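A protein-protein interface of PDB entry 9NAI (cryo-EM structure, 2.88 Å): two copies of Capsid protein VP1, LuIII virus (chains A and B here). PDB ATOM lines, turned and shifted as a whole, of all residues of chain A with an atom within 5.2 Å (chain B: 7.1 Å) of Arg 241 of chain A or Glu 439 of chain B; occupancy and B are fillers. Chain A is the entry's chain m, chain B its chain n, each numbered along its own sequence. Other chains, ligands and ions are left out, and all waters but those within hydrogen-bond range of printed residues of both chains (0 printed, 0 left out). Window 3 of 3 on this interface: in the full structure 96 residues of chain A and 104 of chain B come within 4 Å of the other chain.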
ATOM      1  N   ILE A 100      24.033   7.628  28.860  1.00  0.00           N
ATOM      2  CA  ILE A 100      25.053   6.591  28.870  1.00  0.00           C
ATOM      3  C   ILE A 100      24.959   5.715  27.632  1.00  0.00           C
ATOM      4  O   ILE A 100      25.979   5.358  27.037  1.00  0.00           O
ATOM      5  CB  ILE A 100      24.950   5.779  30.169  1.00  0.00           C
ATOM      6  CG1 ILE A 100      26.067   4.747  30.234  1.00  0.00           C
ATOM      7  CG2 ILE A 100      23.594   5.137  30.305  1.00  0.00           C
ATOM      8  CD1 ILE A 100      26.217   4.118  31.586  1.00  0.00           C
ATOM      9  N   HIS A 101      23.750   5.362  27.212  1.00  0.00           N
ATOM     10  CA  HIS A 101      23.582   4.539  26.028  1.00  0.00           C
ATOM     11  C   HIS A 101      22.249   4.866  25.386  1.00  0.00           C
ATOM     12  O   HIS A 101      21.363   5.447  26.013  1.00  0.00           O
ATOM     13  CB  HIS A 101      23.668   3.051  26.355  1.00  0.00           C
ATOM     14  CG  HIS A 101      22.626   2.583  27.315  1.00  0.00           C
ATOM     15  ND1 HIS A 101      21.318   2.372  26.946  1.00  0.00           N
ATOM     16  CD2 HIS A 101      22.703   2.263  28.626  1.00  0.00           C
ATOM     17  CE1 HIS A 101      20.630   1.955  27.992  1.00  0.00           C
ATOM     18  NE2 HIS A 101      21.448   1.880  29.024  1.00  0.00           N
ATOM     19  N   GLU A 238      20.955  -3.762  18.978  1.00  0.00           N
ATOM     20  CA  GLU A 238      21.600  -3.607  20.271  1.00  0.00           C
ATOM     21  C   GLU A 238      21.877  -2.138  20.549  1.00  0.00           C
ATOM     22  O   GLU A 238      22.293  -1.408  19.651  1.00  0.00           O
ATOM     23  CB  GLU A 238      22.907  -4.377  20.314  1.00  0.00           C
ATOM     24  CG  GLU A 238      22.722  -5.860  20.179  1.00  0.00           C
ATOM     25  CD  GLU A 238      21.810  -6.418  21.246  1.00  0.00           C
ATOM     26  OE1 GLU A 238      21.910  -5.971  22.407  1.00  0.00           O
ATOM     27  OE2 GLU A 238      20.987  -7.300  20.925  1.00  0.00           O
ATOM     28  N   PRO A 239      21.667  -1.676  21.772  1.00  0.00           N
ATOM     29  CA  PRO A 239      21.990  -0.288  22.093  1.00  0.00           C
ATOM     30  C   PRO A 239      23.485  -0.055  22.039  1.00  0.00           C
ATOM     31  O   PRO A 239      24.283  -0.978  22.199  1.00  0.00           O
ATOM     32  CB  PRO A 239      21.454  -0.125  23.514  1.00  0.00           C
ATOM     33  CG  PRO A 239      21.510  -1.485  24.069  1.00  0.00           C
ATOM     34  CD  PRO A 239      21.177  -2.408  22.946  1.00  0.00           C
ATOM     35  N   ILE A 240      23.863   1.194  21.807  1.00  0.00           N
ATOM     36  CA  ILE A 240      25.267   1.564  21.712  1.00  0.00           C
ATOM     37  C   ILE A 240      25.618   2.468  22.876  1.00  0.00           C
ATOM     38  O   ILE A 240      24.792   3.243  23.364  1.00  0.00           O
ATOM     39  CB  ILE A 240      25.603   2.258  20.386  1.00  0.00           C
ATOM     40  CG1 ILE A 240      24.828   3.557  20.273  1.00  0.00           C
ATOM     41  CG2 ILE A 240      25.254   1.366  19.234  1.00  0.00           C
ATOM     42  CD1 ILE A 240      25.253   4.379  19.113  1.00  0.00           C
ATOM     43  N   ARG A 241      26.864   2.374  23.311  1.00  0.00           N
ATOM     44  CA  ARG A 241      27.325   3.083  24.489  1.00  0.00           C
ATOM     45  C   ARG A 241      27.851   4.453  24.098  1.00  0.00           C
ATOM     46  O   ARG A 241      28.619   4.581  23.142  1.00  0.00           O
ATOM     47  CB  ARG A 241      28.403   2.273  25.196  1.00  0.00           C
ATOM     48  CG  ARG A 241      27.898   0.980  25.796  1.00  0.00           C
ATOM     49  CD  ARG A 241      29.027   0.200  26.423  1.00  0.00           C
ATOM     50  NE  ARG A 241      28.576  -1.028  27.051  1.00  0.00           N
ATOM     51  CZ  ARG A 241      28.384  -2.163  26.395  1.00  0.00           C
ATOM     52  NH1 ARG A 241      28.602  -2.218  25.093  1.00  0.00           N
ATOM     53  NH2 ARG A 241      27.973  -3.241  27.040  1.00  0.00           N
ATOM     54  N   LEU A 242      27.431   5.474  24.833  1.00  0.00           N
ATOM     55  CA  LEU A 242      27.763   6.853  24.526  1.00  0.00           C
ATOM     56  C   LEU A 242      28.965   7.379  25.287  1.00  0.00           C
ATOM     57  O   LEU A 242      29.247   8.573  25.210  1.00  0.00           O
ATOM     58  CB  LEU A 242      26.561   7.748  24.783  1.00  0.00           C
ATOM     59  CG  LEU A 242      25.405   7.460  23.840  1.00  0.00           C
ATOM     60  CD1 LEU A 242      24.205   8.282  24.217  1.00  0.00           C
ATOM     61  CD2 LEU A 242      25.832   7.768  22.434  1.00  0.00           C
ATOM     62  N   THR A 243      29.652   6.547  26.054  1.00  0.00           N
ATOM     63  CA  THR A 243      30.785   6.991  26.849  1.00  0.00           C
ATOM     64  C   THR A 243      32.066   6.329  26.367  1.00  0.00           C
ATOM     65  O   THR A 243      32.109   5.113  26.174  1.00  0.00           O
ATOM     66  CB  THR A 243      30.565   6.669  28.317  1.00  0.00           C
ATOM     67  OG1 THR A 243      30.357   5.263  28.454  1.00  0.00           O
ATOM     68  CG2 THR A 243      29.353   7.390  28.828  1.00  0.00           C
ATOM     69  N   PHE A 419      37.621  -4.890  21.943  1.00  0.00           N
ATOM     70  CA  PHE A 419      37.716  -3.533  21.434  1.00  0.00           C
ATOM     71  C   PHE A 419      36.364  -2.863  21.580  1.00  0.00           C
ATOM     72  O   PHE A 419      35.330  -3.535  21.568  1.00  0.00           O
ATOM     73  CB  PHE A 419      38.164  -3.529  19.974  1.00  0.00           C
ATOM     74  CG  PHE A 419      37.283  -4.322  19.089  1.00  0.00           C
ATOM     75  CD1 PHE A 419      36.196  -3.747  18.482  1.00  0.00           C
ATOM     76  CD2 PHE A 419      37.527  -5.655  18.881  1.00  0.00           C
ATOM     77  CE1 PHE A 419      35.382  -4.484  17.677  1.00  0.00           C
ATOM     78  CE2 PHE A 419      36.716  -6.393  18.078  1.00  0.00           C
ATOM     79  CZ  PHE A 419      35.642  -5.808  17.474  1.00  0.00           C
ATOM     80  N   PRO A 420      36.337  -1.547  21.716  1.00  0.00           N
ATOM     81  CA  PRO A 420      35.063  -0.840  21.791  1.00  0.00           C
ATOM     82  C   PRO A 420      34.424  -0.695  20.427  1.00  0.00           C
ATOM     83  O   PRO A 420      35.095  -0.646  19.397  1.00  0.00           O
ATOM     84  CB  PRO A 420      35.459   0.526  22.350  1.00  0.00           C
ATOM     85  CG  PRO A 420      36.824   0.713  21.864  1.00  0.00           C
ATOM     86  CD  PRO A 420      37.473  -0.632  21.876  1.00  0.00           C
ATOM     87  N   HIS A 421      33.122  -0.609  20.439  1.00  0.00           N
ATOM     88  CA  HIS A 421      32.363  -0.398  19.221  1.00  0.00           C
ATOM     89  C   HIS A 421      32.467   1.068  18.828  1.00  0.00           C
ATOM     90  O   HIS A 421      32.235   1.938  19.667  1.00  0.00           O
ATOM     91  CB  HIS A 421      30.919  -0.784  19.466  1.00  0.00           C
ATOM     92  CG  HIS A 421      30.064  -0.780  18.247  1.00  0.00           C
ATOM     93  ND1 HIS A 421      28.691  -0.731  18.313  1.00  0.00           N
ATOM     94  CD2 HIS A 421      30.372  -0.890  16.938  1.00  0.00           C
ATOM     95  CE1 HIS A 421      28.192  -0.769  17.093  1.00  0.00           C
ATOM     96  NE2 HIS A 421      29.193  -0.864  16.239  1.00  0.00           N
ATOM     97  N   ARG A 544      30.769  11.100  22.460  1.00  0.00           N
ATOM     98  CA  ARG A 544      31.172  10.360  23.645  1.00  0.00           C
ATOM     99  C   ARG A 544      32.073  11.201  24.530  1.00  0.00           C
ATOM    100  O   ARG A 544      33.241  10.856  24.729  1.00  0.00           O
ATOM    101  CB  ARG A 544      31.884   9.068  23.260  1.00  0.00           C
ATOM    102  CG  ARG A 544      30.994   8.051  22.610  1.00  0.00           C
ATOM    103  CD  ARG A 544      31.767   6.803  22.288  1.00  0.00           C
ATOM    104  NE  ARG A 544      30.929   5.796  21.658  1.00  0.00           N
ATOM    105  CZ  ARG A 544      31.389   4.661  21.155  1.00  0.00           C
ATOM    106  NH1 ARG A 544      32.684   4.396  21.194  1.00  0.00           N
ATOM    107  NH2 ARG A 544      30.559   3.795  20.604  1.00  0.00           N
ATOM    108  N   ARG A 548      34.501   6.501  30.900  1.00  0.00           N
ATOM    109  CA  ARG A 548      33.873   5.353  31.519  1.00  0.00           C
ATOM    110  C   ARG A 548      34.951   4.406  32.000  1.00  0.00           C
ATOM    111  O   ARG A 548      36.027   4.321  31.410  1.00  0.00           O
ATOM    112  CB  ARG A 548      32.962   4.645  30.536  1.00  0.00           C
ATOM    113  CG  ARG A 548      32.261   3.454  31.093  1.00  0.00           C
ATOM    114  CD  ARG A 548      31.424   2.869  30.016  1.00  0.00           C
ATOM    115  NE  ARG A 548      32.203   2.295  28.931  1.00  0.00           N
ATOM    116  CZ  ARG A 548      31.721   2.166  27.706  1.00  0.00           C
ATOM    117  NH1 ARG A 548      30.525   2.646  27.446  1.00  0.00           N
ATOM    118  NH2 ARG A 548      32.432   1.621  26.739  1.00  0.00           N
ATOM    119  N   LEU B 436      34.849  -7.192  30.887  1.00  0.00           N
ATOM    120  CA  LEU B 436      35.085  -5.835  30.428  1.00  0.00           C
ATOM    121  C   LEU B 436      33.792  -5.227  29.911  1.00  0.00           C
ATOM    122  O   LEU B 436      32.889  -5.928  29.457  1.00  0.00           O
ATOM    123  CB  LEU B 436      36.136  -5.826  29.329  1.00  0.00           C
ATOM    124  CG  LEU B 436      37.596  -5.859  29.765  1.00  0.00           C
ATOM    125  CD1 LEU B 436      37.939  -7.170  30.418  1.00  0.00           C
ATOM    126  CD2 LEU B 436      38.483  -5.628  28.574  1.00  0.00           C
ATOM    127  N   ASP B 437      33.710  -3.905  29.975  1.00  0.00           N
ATOM    128  CA  ASP B 437      32.496  -3.197  29.608  1.00  0.00           C
ATOM    129  C   ASP B 437      32.484  -2.834  28.131  1.00  0.00           C
ATOM    130  O   ASP B 437      31.573  -2.144  27.670  1.00  0.00           O
ATOM    131  CB  ASP B 437      32.347  -1.947  30.474  1.00  0.00           C
ATOM    132  CG  ASP B 437      30.969  -1.312  30.375  1.00  0.00           C
ATOM    133  OD1 ASP B 437      30.076  -1.878  29.715  1.00  0.00           O
ATOM    134  OD2 ASP B 437      30.779  -0.233  30.969  1.00  0.00           O
ATOM    135  N   LEU B 438      33.482  -3.274  27.382  1.00  0.00           N
ATOM    136  CA  LEU B 438      33.499  -3.027  25.956  1.00  0.00           C
ATOM    137  C   LEU B 438      32.343  -3.749  25.284  1.00  0.00           C
ATOM    138  O   LEU B 438      31.796  -4.721  25.804  1.00  0.00           O
ATOM    139  CB  LEU B 438      34.820  -3.491  25.366  1.00  0.00           C
ATOM    140  CG  LEU B 438      35.974  -2.712  25.970  1.00  0.00           C
ATOM    141  CD1 LEU B 438      37.292  -3.254  25.487  1.00  0.00           C
ATOM    142  CD2 LEU B 438      35.825  -1.259  25.616  1.00  0.00           C
ATOM    143  N   GLU B 439      31.957  -3.249  24.115  1.00  0.00           N
ATOM    144  CA  GLU B 439      30.889  -3.893  23.364  1.00  0.00           C
ATOM    145  C   GLU B 439      31.303  -5.264  22.869  1.00  0.00           C
ATOM    146  O   GLU B 439      30.549  -6.232  22.993  1.00  0.00           O
ATOM    147  CB  GLU B 439      30.467  -3.024  22.191  1.00  0.00           C
ATOM    148  CG  GLU B 439      29.412  -3.679  21.334  1.00  0.00           C
ATOM    149  CD  GLU B 439      28.115  -3.926  22.072  1.00  0.00           C
ATOM    150  OE1 GLU B 439      27.914  -3.352  23.162  1.00  0.00           O
ATOM    151  OE2 GLU B 439      27.293  -4.715  21.565  1.00  0.00           O
ATOM    152  N   HIS B 440      32.484  -5.366  22.290  1.00  0.00           N
ATOM    153  CA  HIS B 440      32.935  -6.603  21.682  1.00  0.00           C
ATOM    154  C   HIS B 440      33.915  -7.271  22.626  1.00  0.00           C
ATOM    155  O   HIS B 440      34.966  -6.707  22.938  1.00  0.00           O
ATOM    156  CB  HIS B 440      33.559  -6.317  20.327  1.00  0.00           C
ATOM    157  CG  HIS B 440      32.589  -5.712  19.371  1.00  0.00           C
ATOM    158  ND1 HIS B 440      32.318  -4.363  19.352  1.00  0.00           N
ATOM    159  CD2 HIS B 440      31.772  -6.273  18.453  1.00  0.00           C
ATOM    160  CE1 HIS B 440      31.403  -4.115  18.435  1.00  0.00           C
ATOM    161  NE2 HIS B 440      31.055  -5.257  17.875  1.00  0.00           N
ATOM    162  N   LYS B 441      33.589  -8.460  23.045  1.00  0.00           N
ATOM    163  CA  LYS B 441      34.227  -9.000  24.215  1.00  0.00           C
ATOM    164  C   LYS B 441      35.106 -10.176  23.848  1.00  0.00           C
ATOM    165  O   LYS B 441      34.851 -10.865  22.860  1.00  0.00           O
ATOM    166  CB  LYS B 441      33.168  -9.460  25.218  1.00  0.00           C
ATOM    167  CG  LYS B 441      32.340  -8.337  25.770  1.00  0.00           C
ATOM    168  CD  LYS B 441      31.353  -8.842  26.785  1.00  0.00           C
ATOM    169  CE  LYS B 441      30.621  -7.694  27.437  1.00  0.00           C
ATOM    170  NZ  LYS B 441      29.609  -7.111  26.523  1.00  0.00           N
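Arg 241 of chain A touches just these residues of chain B: Asp 437 and Glu 439. Printed residues of chain A within 4 Å of Asp 437 of chain B: Arg 241 (3.2 Å) and Arg 548 (3.3 Å). Of the printed residues of chain B, Arg 548 of chain A touches Asp 437 (3.3 Å). Lys 441 of chain B touches none of the printed residues of chain A. The nearest printed residue of chain A that does not touch Asp 437 of chain B is Thr 243 of chain A (6.1 Å).
Among the printed residues, merely in contact across the chains: Phe 419 of chain A with Leu 438 of chain B (3.8 Å), Pro 420 of chain A with Leu 438 of chain B (3.7 Å), His 421 of chain A with Glu 439 of chain B (3.6 Å) and His 421 of chain A with His 440 of chain B (3.5 Å).
The side-chain hydroxyl (OG1) of Thr 243 of chain A sits at hydrogen-bond distance from the guanidinium group (NH1) of Arg 548 of chain A (2.8 Å). The backbone carbonyl oxygen of Arg 241 of chain A lies within hydrogen-bond range of the guanidinium group of Arg 544 of chain A. NH2 of Arg 544 of chain A sits at hydrogen-bond distance from O of His 421 of chain A (2.7 Å). The backbone carbonyl oxygen of Leu 438 of chain B is in hydrogen-bond range of the side-chain amino group of Lys 441 of chain B (3.3 Å).
Along chain B the printed residues that touch a printed residue of chain A span positions 437 to 440. Among the printed residues, Asp or Glu carboxylates within 4 Å of a Lys or Arg side-chain nitrogen of the other chain: Arg 241 of chain A with Asp 437 of chain B, Arg 241 of chain A with Glu 439 of chain B and Arg 548 of chain A with Asp 437 of chain B.
The guanidinium group of Arg 241 of chain A is in salt-bridge range of the side-chain carboxylate of Asp 437 of chain B (3.2 Å). NE of Arg 548 of chain A lies within salt-bridge range of OD2 of Asp 437 of chain B (3.5 Å). The guanidinium group of Arg 241 of chain A lies within salt-bridge range of the side-chain carboxylate of Glu 439 of chain B. The backbone carbonyl oxygen (O) of His 440 of chain B sits at hydrogen-bond distance from the backbone NH (N) of Phe 419 of chain A.
No position is printed for both chains.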
